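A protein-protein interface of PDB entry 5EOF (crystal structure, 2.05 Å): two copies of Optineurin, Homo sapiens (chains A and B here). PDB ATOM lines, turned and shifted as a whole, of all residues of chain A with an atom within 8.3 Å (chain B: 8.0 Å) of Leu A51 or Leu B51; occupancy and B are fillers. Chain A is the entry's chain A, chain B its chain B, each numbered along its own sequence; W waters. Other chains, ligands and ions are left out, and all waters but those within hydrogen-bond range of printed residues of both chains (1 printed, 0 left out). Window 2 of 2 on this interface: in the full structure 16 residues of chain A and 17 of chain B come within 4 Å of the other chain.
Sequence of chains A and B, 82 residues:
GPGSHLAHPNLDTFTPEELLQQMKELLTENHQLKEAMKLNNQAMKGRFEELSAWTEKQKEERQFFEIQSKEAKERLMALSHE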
ATOM      1  N   MET A  44      18.226  19.144  23.463  1.00  0.00           N
ATOM      2  CA  MET A  44      17.400  20.314  23.765  1.00  0.00           C
ATOM      3  C   MET A  44      18.253  21.581  23.888  1.00  0.00           C
ATOM      4  O   MET A  44      17.829  22.668  23.484  1.00  0.00           O
ATOM      5  CB  MET A  44      16.582  20.101  25.035  1.00  0.00           C
ATOM      6  CG  MET A  44      15.441  19.118  24.844  1.00  0.00           C
ATOM      7  SD  MET A  44      13.989  19.964  24.218  1.00  0.00           S
ATOM      8  CE  MET A  44      13.450  20.707  25.753  1.00  0.00           C
ATOM      9  N   LYS A  45      19.458  21.435  24.426  1.00  0.00           N
ATOM     10  CA  LYS A  45      20.374  22.563  24.509  1.00  0.00           C
ATOM     11  C   LYS A  45      20.790  22.991  23.107  1.00  0.00           C
ATOM     12  O   LYS A  45      20.974  24.163  22.862  1.00  0.00           O
ATOM     13  CB  LYS A  45      21.611  22.226  25.330  1.00  0.00           C
ATOM     14  CG  LYS A  45      21.328  21.992  26.828  1.00  0.00           C
ATOM     15  CD  LYS A  45      22.645  21.814  27.588  1.00  0.00           C
ATOM     16  CE  LYS A  45      22.407  21.238  28.983  1.00  0.00           C
ATOM     17  NZ  LYS A  45      23.690  20.961  29.706  1.00  0.00           N
ATOM     18  N   GLY A  46      20.951  22.032  22.202  1.00  0.00           N
ATOM     19  CA  GLY A  46      21.252  22.341  20.813  1.00  0.00           C
ATOM     20  C   GLY A  46      20.098  23.058  20.146  1.00  0.00           C
ATOM     21  O   GLY A  46      20.309  24.089  19.490  1.00  0.00           O
ATOM     22  N   ARG A  47      18.884  22.518  20.288  1.00  0.00           N
ATOM     23  CA  ARG A  47      17.686  23.166  19.730  1.00  0.00           C
ATOM     24  C   ARG A  47      17.542  24.595  20.229  1.00  0.00           C
ATOM     25  O   ARG A  47      17.128  25.485  19.472  1.00  0.00           O
ATOM     26  CB  ARG A  47      16.401  22.390  20.044  1.00  0.00           C
ATOM     27  CG  ARG A  47      16.366  20.930  19.546  1.00  0.00           C
ATOM     28  CD  ARG A  47      16.546  20.831  18.008  1.00  0.00           C
ATOM     29  NE  ARG A  47      17.961  20.803  17.648  1.00  0.00           N
ATOM     30  CZ  ARG A  47      18.743  19.739  17.777  1.00  0.00           C
ATOM     31  NH1 ARG A  47      20.020  19.821  17.440  1.00  0.00           N
ATOM     32  NH2 ARG A  47      18.249  18.591  18.247  1.00  0.00           N
ATOM     33  N   PHE A  48      17.891  24.818  21.494  1.00  0.00           N
ATOM     34  CA  PHE A  48      17.818  26.149  22.088  1.00  0.00           C
ATOM     35  C   PHE A  48      18.810  27.131  21.447  1.00  0.00           C
ATOM     36  O   PHE A  48      18.449  28.276  21.189  1.00  0.00           O
ATOM     37  CB  PHE A  48      18.036  26.092  23.608  1.00  0.00           C
ATOM     38  CG  PHE A  48      17.961  27.437  24.290  1.00  0.00           C
ATOM     39  CD1 PHE A  48      19.080  28.243  24.387  1.00  0.00           C
ATOM     40  CD2 PHE A  48      16.771  27.889  24.834  1.00  0.00           C
ATOM     41  CE1 PHE A  48      19.017  29.481  25.025  1.00  0.00           C
ATOM     42  CE2 PHE A  48      16.699  29.110  25.475  1.00  0.00           C
ATOM     43  CZ  PHE A  48      17.826  29.910  25.570  1.00  0.00           C
ATOM     44  N   GLU A  49      20.053  26.708  21.226  1.00  0.00           N
ATOM     45  CA  GLU A  49      21.033  27.600  20.600  1.00  0.00           C
ATOM     46  C   GLU A  49      20.630  27.893  19.168  1.00  0.00           C
ATOM     47  O   GLU A  49      20.768  29.018  18.694  1.00  0.00           O
ATOM     48  CB  GLU A  49      22.429  26.982  20.607  1.00  0.00           C
ATOM     49  CG  GLU A  49      22.975  26.678  21.987  1.00  0.00           C
ATOM     50  CD  GLU A  49      23.009  27.887  22.913  1.00  0.00           C
ATOM     51  OE1 GLU A  49      23.265  29.013  22.440  1.00  0.00           O
ATOM     52  OE2 GLU A  49      22.787  27.707  24.128  1.00  0.00           O
ATOM     53  N   GLU A  50      20.137  26.870  18.479  1.00  0.00           N
ATOM     54  CA  GLU A  50      19.656  27.015  17.100  1.00  0.00           C
ATOM     55  C   GLU A  50      18.523  28.024  16.986  1.00  0.00           C
ATOM     56  O   GLU A  50      18.537  28.909  16.108  1.00  0.00           O
ATOM     57  CB  GLU A  50      19.208  25.654  16.547  1.00  0.00           C
ATOM     58  CG  GLU A  50      20.364  24.731  16.200  1.00  0.00           C
ATOM     59  CD  GLU A  50      19.965  23.242  16.206  1.00  0.00           C
ATOM     60  OE1 GLU A  50      20.865  22.394  16.314  1.00  0.00           O
ATOM     61  OE2 GLU A  50      18.758  22.915  16.103  1.00  0.00           O
ATOM     62  N   LEU A  51      17.532  27.891  17.853  1.00  0.00           N
ATOM     63  CA  LEU A  51      16.402  28.799  17.844  1.00  0.00           C
ATOM     64  C   LEU A  51      16.829  30.231  18.201  1.00  0.00           C
ATOM     65  O   LEU A  51      16.329  31.179  17.606  1.00  0.00           O
ATOM     66  CB  LEU A  51      15.273  28.294  18.746  1.00  0.00           C
ATOM     67  CG  LEU A  51      14.504  27.100  18.162  1.00  0.00           C
ATOM     68  CD1 LEU A  51      13.824  26.273  19.232  1.00  0.00           C
ATOM     69  CD2 LEU A  51      13.467  27.586  17.159  1.00  0.00           C
ATOM     70  N   SER A  52      17.772  30.383  19.134  1.00  0.00           N
ATOM     71  CA  SER A  52      18.309  31.707  19.486  1.00  0.00           C
ATOM     72  C   SER A  52      19.049  32.351  18.322  1.00  0.00           C
ATOM     73  O   SER A  52      18.836  33.519  18.009  1.00  0.00           O
ATOM     74  CB  SER A  52      19.273  31.614  20.667  1.00  0.00           C
ATOM     75  OG  SER A  52      18.659  31.024  21.790  1.00  0.00           O
ATOM     76  N   ALA A  53      19.946  31.598  17.698  1.00  0.00           N
ATOM     77  CA  ALA A  53      20.636  32.100  16.525  1.00  0.00           C
ATOM     78  C   ALA A  53      19.643  32.478  15.413  1.00  0.00           C
ATOM     79  O   ALA A  53      19.792  33.521  14.752  1.00  0.00           O
ATOM     80  CB  ALA A  53      21.670  31.098  16.039  1.00  0.00           C
ATOM     81  N   TRP A  54      18.604  31.666  15.236  1.00  0.00           N
ATOM     82  CA  TRP A  54      17.633  31.878  14.163  1.00  0.00           C
ATOM     83  C   TRP A  54      16.818  33.141  14.369  1.00  0.00           C
ATOM     84  O   TRP A  54      16.589  33.903  13.419  1.00  0.00           O
ATOM     85  CB  TRP A  54      16.688  30.679  14.034  1.00  0.00           C
ATOM     86  CG  TRP A  54      15.634  30.798  12.931  1.00  0.00           C
ATOM     87  CD1 TRP A  54      15.773  30.430  11.618  1.00  0.00           C
ATOM     88  CD2 TRP A  54      14.285  31.277  13.067  1.00  0.00           C
ATOM     89  NE1 TRP A  54      14.599  30.651  10.936  1.00  0.00           N
ATOM     90  CE2 TRP A  54      13.669  31.176  11.802  1.00  0.00           C
ATOM     91  CE3 TRP A  54      13.535  31.783  14.140  1.00  0.00           C
ATOM     92  CZ2 TRP A  54      12.345  31.558  11.575  1.00  0.00           C
ATOM     93  CZ3 TRP A  54      12.219  32.166  13.913  1.00  0.00           C
ATOM     94  CH2 TRP A  54      11.639  32.050  12.640  1.00  0.00           C
ATOM     95  N   THR A  55      16.364  33.353  15.604  1.00  0.00           N
ATOM     96  CA  THR A  55      15.570  34.542  15.894  1.00  0.00           C
ATOM     97  C   THR A  55      16.403  35.820  15.713  1.00  0.00           C
ATOM     98  O   THR A  55      15.893  36.841  15.252  1.00  0.00           O
ATOM     99  CB  THR A  55      14.906  34.473  17.293  1.00  0.00           C
ATOM    100  OG1 THR A  55      14.054  35.606  17.482  1.00  0.00           O
ATOM    101  CG2 THR A  55      15.938  34.464  18.397  1.00  0.00           C
ATOM    102  N   GLU A  56      17.688  35.758  16.053  1.00  0.00           N
ATOM    103  CA  GLU A  56      18.584  36.885  15.793  1.00  0.00           C
ATOM    104  C   GLU A  56      18.735  37.175  14.304  1.00  0.00           C
ATOM    105  O   GLU A  56      18.737  38.339  13.876  1.00  0.00           O
ATOM    106  CB  GLU A  56      19.954  36.631  16.424  1.00  0.00           C
ATOM    107  CG  GLU A  56      20.135  37.292  17.781  1.00  0.00           C
ATOM    108  CD  GLU A  56      18.921  37.129  18.685  1.00  0.00           C
ATOM    109  OE1 GLU A  56      18.071  38.049  18.713  1.00  0.00           O
ATOM    110  OE2 GLU A  56      18.817  36.081  19.367  1.00  0.00           O
ATOM    111  N   LYS A  57      18.879  36.119  13.513  1.00  0.00           N
ATOM    112  CA  LYS A  57      18.970  36.277  12.071  1.00  0.00           C
ATOM    113  C   LYS A  57      17.689  36.891  11.543  1.00  0.00           C
ATOM    114  O   LYS A  57      17.741  37.808  10.720  1.00  0.00           O
ATOM    115  CB  LYS A  57      19.272  34.947  11.365  1.00  0.00           C
ATOM    116  CG  LYS A  57      19.251  35.031   9.827  1.00  0.00           C
ATOM    117  CD  LYS A  57      19.702  33.730   9.139  1.00  0.00           C
ATOM    118  CE  LYS A  57      18.745  32.551   9.397  1.00  0.00           C
ATOM    119  NZ  LYS A  57      17.411  32.608   8.708  1.00  0.00           N
ATOM    120  N   GLN A  58      16.539  36.416  12.020  1.00  0.00           N
ATOM    121  CA  GLN A  58      15.264  36.955  11.532  1.00  0.00           C
ATOM    122  C   GLN A  58      15.119  38.454  11.812  1.00  0.00           C
ATOM    123  O   GLN A  58      14.699  39.214  10.942  1.00  0.00           O
ATOM    124  CB  GLN A  58      14.074  36.205  12.123  1.00  0.00           C
ATOM    125  CG  GLN A  58      14.036  34.749  11.718  1.00  0.00           C
ATOM    126  CD  GLN A  58      13.975  34.587  10.229  1.00  0.00           C
ATOM    127  OE1 GLN A  58      13.022  35.025   9.594  1.00  0.00           O
ATOM    128  NE2 GLN A  58      14.998  33.963   9.652  1.00  0.00           N
ATOM    129  N   MET B  44       6.713  20.039  27.669  1.00  0.00           N
ATOM    130  CA  MET B  44       7.330  19.907  26.344  1.00  0.00           C
ATOM    131  C   MET B  44       6.361  20.360  25.268  1.00  0.00           C
ATOM    132  O   MET B  44       6.722  21.099  24.335  1.00  0.00           O
ATOM    133  CB  MET B  44       7.713  18.456  26.054  1.00  0.00           C
ATOM    134  CG  MET B  44       9.092  18.043  26.548  1.00  0.00           C
ATOM    135  SD  MET B  44      10.433  18.744  25.567  1.00  0.00           S
ATOM    136  CE  MET B  44      10.362  17.726  24.095  1.00  0.00           C
ATOM    137  N   LYS B  45       5.121  19.908  25.406  1.00  0.00           N
ATOM    138  CA  LYS B  45       4.083  20.164  24.413  1.00  0.00           C
ATOM    139  C   LYS B  45       3.694  21.644  24.426  1.00  0.00           C
ATOM    140  O   LYS B  45       3.481  22.248  23.373  1.00  0.00           O
ATOM    141  CB  LYS B  45       2.874  19.255  24.694  1.00  0.00           C
ATOM    142  CG  LYS B  45       1.717  19.405  23.726  1.00  0.00           C
ATOM    143  CD  LYS B  45       0.747  18.222  23.827  1.00  0.00           C
ATOM    144  CE  LYS B  45      -0.399  18.341  22.799  1.00  0.00           C
ATOM    145  NZ  LYS B  45      -1.712  18.785  23.382  1.00  0.00           N
ATOM    146  N   GLY B  46       3.604  22.219  25.626  1.00  0.00           N
ATOM    147  CA  GLY B  46       3.289  23.625  25.792  1.00  0.00           C
ATOM    148  C   GLY B  46       4.365  24.504  25.183  1.00  0.00           C
ATOM    149  O   GLY B  46       4.060  25.456  24.452  1.00  0.00           O
ATOM    150  N   ARG B  47       5.628  24.188  25.468  1.00  0.00           N
ATOM    151  CA  ARG B  47       6.722  24.927  24.846  1.00  0.00           C
ATOM    152  C   ARG B  47       6.736  24.761  23.322  1.00  0.00           C
ATOM    153  O   ARG B  47       6.957  25.737  22.615  1.00  0.00           O
ATOM    154  CB  ARG B  47       8.079  24.546  25.429  1.00  0.00           C
ATOM    155  CG  ARG B  47       8.245  24.886  26.903  1.00  0.00           C
ATOM    156  CD  ARG B  47       7.972  26.355  27.208  1.00  0.00           C
ATOM    157  NE  ARG B  47       8.245  26.626  28.620  1.00  0.00           N
ATOM    158  CZ  ARG B  47       7.599  27.522  29.361  1.00  0.00           C
ATOM    159  NH1 ARG B  47       6.627  28.256  28.825  1.00  0.00           N
ATOM    160  NH2 ARG B  47       7.933  27.686  30.640  1.00  0.00           N
ATOM    161  N   PHE B  48       6.523  23.540  22.823  1.00  0.00           N
ATOM    162  CA  PHE B  48       6.515  23.316  21.386  1.00  0.00           C
ATOM    163  C   PHE B  48       5.440  24.196  20.757  1.00  0.00           C
ATOM    164  O   PHE B  48       5.683  24.814  19.725  1.00  0.00           O
ATOM    165  CB  PHE B  48       6.286  21.855  20.986  1.00  0.00           C
ATOM    166  CG  PHE B  48       6.230  21.652  19.483  1.00  0.00           C
ATOM    167  CD1 PHE B  48       7.397  21.491  18.745  1.00  0.00           C
ATOM    168  CD2 PHE B  48       5.016  21.681  18.802  1.00  0.00           C
ATOM    169  CE1 PHE B  48       7.356  21.338  17.353  1.00  0.00           C
ATOM    170  CE2 PHE B  48       4.971  21.531  17.418  1.00  0.00           C
ATOM    171  CZ  PHE B  48       6.143  21.356  16.692  1.00  0.00           C
ATOM    172  N   GLU B  49       4.266  24.260  21.381  1.00  0.00           N
ATOM    173  CA  GLU B  49       3.185  25.077  20.847  1.00  0.00           C
ATOM    174  C   GLU B  49       3.569  26.563  20.838  1.00  0.00           C
ATOM    175  O   GLU B  49       3.311  27.265  19.862  1.00  0.00           O
ATOM    176  CB  GLU B  49       1.898  24.863  21.639  1.00  0.00           C
ATOM    177  CG  GLU B  49       1.230  23.520  21.402  1.00  0.00           C
ATOM    178  CD  GLU B  49       0.181  23.196  22.461  1.00  0.00           C
ATOM    179  OE1 GLU B  49      -0.018  24.023  23.382  1.00  0.00           O
ATOM    180  OE2 GLU B  49      -0.443  22.117  22.372  1.00  0.00           O
ATOM    181  N   GLU B  50       4.204  27.027  21.914  1.00  0.00           N
ATOM    182  CA  GLU B  50       4.591  28.434  22.027  1.00  0.00           C
ATOM    183  C   GLU B  50       5.675  28.786  21.031  1.00  0.00           C
ATOM    184  O   GLU B  50       5.660  29.872  20.456  1.00  0.00           O
ATOM    185  CB  GLU B  50       5.103  28.757  23.433  1.00  0.00           C
ATOM    186  CG  GLU B  50       4.058  28.736  24.516  1.00  0.00           C
ATOM    187  CD  GLU B  50       4.687  28.593  25.907  1.00  0.00           C
ATOM    188  OE1 GLU B  50       5.937  28.716  26.025  1.00  0.00           O
ATOM    189  OE2 GLU B  50       3.935  28.350  26.876  1.00  0.00           O
ATOM    190  N   LEU B  51       6.626  27.878  20.831  1.00  0.00           N
ATOM    191  CA  LEU B  51       7.717  28.151  19.906  1.00  0.00           C
ATOM    192  C   LEU B  51       7.242  28.147  18.460  1.00  0.00           C
ATOM    193  O   LEU B  51       7.736  28.924  17.642  1.00  0.00           O
ATOM    194  CB  LEU B  51       8.856  27.161  20.075  1.00  0.00           C
ATOM    195  CG  LEU B  51       9.644  27.262  21.379  1.00  0.00           C
ATOM    196  CD1 LEU B  51      10.575  26.101  21.410  1.00  0.00           C
ATOM    197  CD2 LEU B  51      10.426  28.561  21.461  1.00  0.00           C
ATOM    198  N   SER B  52       6.281  27.276  18.156  1.00  0.00           N
ATOM    199  CA  SER B  52       5.682  27.222  16.824  1.00  0.00           C
ATOM    200  C   SER B  52       5.034  28.554  16.486  1.00  0.00           C
ATOM    201  O   SER B  52       5.315  29.155  15.435  1.00  0.00           O
ATOM    202  CB  SER B  52       4.623  26.115  16.740  1.00  0.00           C
ATOM    203  OG  SER B  52       5.211  24.841  16.875  1.00  0.00           O
ATOM    204  N   ALA B  53       4.165  29.011  17.381  1.00  0.00           N
ATOM    205  CA  ALA B  53       3.484  30.285  17.229  1.00  0.00           C
ATOM    206  C   ALA B  53       4.491  31.429  17.049  1.00  0.00           C
ATOM    207  O   ALA B  53       4.338  32.291  16.183  1.00  0.00           O
ATOM    208  CB  ALA B  53       2.600  30.542  18.429  1.00  0.00           C
ATOM    209  N   TRP B  54       5.530  31.407  17.874  1.00  0.00           N
ATOM    210  CA  TRP B  54       6.559  32.441  17.895  1.00  0.00           C
ATOM    211  C   TRP B  54       7.398  32.462  16.625  1.00  0.00           C
ATOM    212  O   TRP B  54       7.617  33.537  16.037  1.00  0.00           O
ATOM    213  CB  TRP B  54       7.429  32.225  19.128  1.00  0.00           C
ATOM    214  CG  TRP B  54       8.593  33.134  19.317  1.00  0.00           C
ATOM    215  CD1 TRP B  54       8.571  34.444  19.719  1.00  0.00           C
ATOM    216  CD2 TRP B  54       9.971  32.770  19.206  1.00  0.00           C
ATOM    217  NE1 TRP B  54       9.859  34.921  19.834  1.00  0.00           N
ATOM    218  CE2 TRP B  54      10.735  33.910  19.532  1.00  0.00           C
ATOM    219  CE3 TRP B  54      10.636  31.585  18.865  1.00  0.00           C
ATOM    220  CZ2 TRP B  54      12.135  33.901  19.517  1.00  0.00           C
ATOM    221  CZ3 TRP B  54      12.023  31.576  18.848  1.00  0.00           C
ATOM    222  CH2 TRP B  54      12.759  32.730  19.175  1.00  0.00           C
ATOM    223  N   THR B  55       7.863  31.296  16.181  1.00  0.00           N
ATOM    224  CA  THR B  55       8.615  31.251  14.922  1.00  0.00           C
ATOM    225  C   THR B  55       7.745  31.702  13.742  1.00  0.00           C
ATOM    226  O   THR B  55       8.216  32.396  12.826  1.00  0.00           O
ATOM    227  CB  THR B  55       9.209  29.862  14.629  1.00  0.00           C
ATOM    228  OG1 THR B  55       8.156  28.898  14.630  1.00  0.00           O
ATOM    229  CG2 THR B  55      10.249  29.480  15.686  1.00  0.00           C
ATOM    230  N   GLU B  56       6.478  31.304  13.762  1.00  0.00           N
ATOM    231  CA  GLU B  56       5.559  31.689  12.695  1.00  0.00           C
ATOM    232  C   GLU B  56       5.377  33.201  12.651  1.00  0.00           C
ATOM    233  O   GLU B  56       5.365  33.806  11.577  1.00  0.00           O
ATOM    234  CB  GLU B  56       4.198  31.004  12.871  1.00  0.00           C
ATOM    235  CG  GLU B  56       3.335  31.009  11.611  1.00  0.00           C
ATOM    236  CD  GLU B  56       4.013  30.307  10.440  1.00  0.00           C
ATOM    237  OE1 GLU B  56       4.592  29.215  10.649  1.00  0.00           O
ATOM    238  OE2 GLU B  56       3.976  30.851   9.314  1.00  0.00           O
ATOM    239  N   LYS B  57       5.232  33.812  13.818  1.00  0.00           N
ATOM    240  CA  LYS B  57       5.035  35.246  13.889  1.00  0.00           C
ATOM    241  C   LYS B  57       6.221  35.965  13.247  1.00  0.00           C
ATOM    242  O   LYS B  57       6.036  36.881  12.457  1.00  0.00           O
ATOM    243  CB  LYS B  57       4.841  35.703  15.334  1.00  0.00           C
ATOM    244  CG  LYS B  57       4.342  37.137  15.444  1.00  0.00           C
ATOM    245  CD  LYS B  57       4.315  37.631  16.886  1.00  0.00           C
ATOM    246  CE  LYS B  57       5.720  37.733  17.473  1.00  0.00           C
ATOM    247  NZ  LYS B  57       6.613  38.631  16.676  1.00  0.00           N
ATOM    248  N   GLN B  58       7.435  35.519  13.548  1.00  0.00           N
ATOM    249  CA  GLN B  58       8.627  36.164  13.007  1.00  0.00           C
ATOM    250  C   GLN B  58       8.802  36.000  11.503  1.00  0.00           C
ATOM    251  O   GLN B  58       9.348  36.894  10.850  1.00  0.00           O
ATOM    252  CB  GLN B  58       9.871  35.664  13.729  1.00  0.00           C
ATOM    253  CG  GLN B  58       9.740  35.764  15.229  1.00  0.00           C
ATOM    254  CD  GLN B  58      10.993  36.283  15.849  1.00  0.00           C
ATOM    255  OE1 GLN B  58      12.044  35.638  15.788  1.00  0.00           O
ATOM    256  NE2 GLN B  58      10.910  37.478  16.428  1.00  0.00           N
HETATM  257  O   HOH W   1      13.452  16.717  26.077  1.00  0.00           O
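Among the printed residues, merely in contact across the chains: Thr A55 with Trp B54, Trp A54 with Thr B55, Met A44 with Met B44, Leu A51 with Leu B51 and Trp A54 with Gln B58.
The side-chain amide oxygen (OE1) of Gln B58 is in hydrogen-bond range of the side-chain hydroxyl (OG1) of Thr A55 (2.6 Å).
Water W1 lies within hydrogen-bond range of the side-chain sulfur of Met B44 (3.7 Å) and the side-chain sulfur of Met A44 (3.8 Å).
Printed residues of chain B within 4 Å of Leu A51: Leu B51 (3.9 Å).
Of the printed residues of chain A, Leu B51 touches Leu A51 (3.9 Å).
Printed residues of chain B within 4 Å of Thr A55: Trp B54 and Gln B58.
Of the printed residues of chain A, Gln B58 touches Trp A54 and Thr A55.
The nearest printed residue of chain B that does not touch Leu A51 is Thr B55 (4.01 Å).
The nearest printed residue of chain A that does not touch Leu B51 is Trp A54 (6.7 Å).
The backbone carbonyl oxygen of Ser B52 lies within hydrogen-bond range of the side-chain hydroxyl of Thr B55, at 3.0 Å.
O of Leu B51 is in hydrogen-bond range of OG1 of Thr B55, 3.0 Å away.
Printed residues of chain B that touch a printed residue of chain A: Met B44, Leu B51, Trp B54, Thr B55 and Gln B58.
Hydrophobic or aromatic side chains of chain B that line the printed part of chain A: Met B44, Leu B51 and Trp B54.
Of the 15 printed residues of chain A, 4 touch a printed residue of chain B.
Printed residues of chain A that touch a printed residue of chain B: Met A44, Leu A51, Trp A54 and Thr A55.
Hydrophobic or aromatic side chains of chain A that line the printed part of chain B: Met A44, Leu A51 and Trp A54.
Along chain A the printed residues that touch a printed residue of chain B span positions 44 to 55.
Among the printed residues, no Asp or Glu carboxylate lies within 4 Å of a Lys or Arg side-chain nitrogen of the other chain.
Met A44 touches its own counterpart, Met B44.
Leu A51 touches its own counterpart, Leu B51.
Trp A54 touches Thr B55, and with the chains exchanged Thr A55 touches Trp B54.
Thr A55 touches Gln B58, but with the chains exchanged Gln A58 does not touch Thr B55 (6.4 Å).
Positions printed for both chains: 44, 45, 46, 47, 48, 49, 50, 51, 52, 53, 54, 55, 56, 57 and 58.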
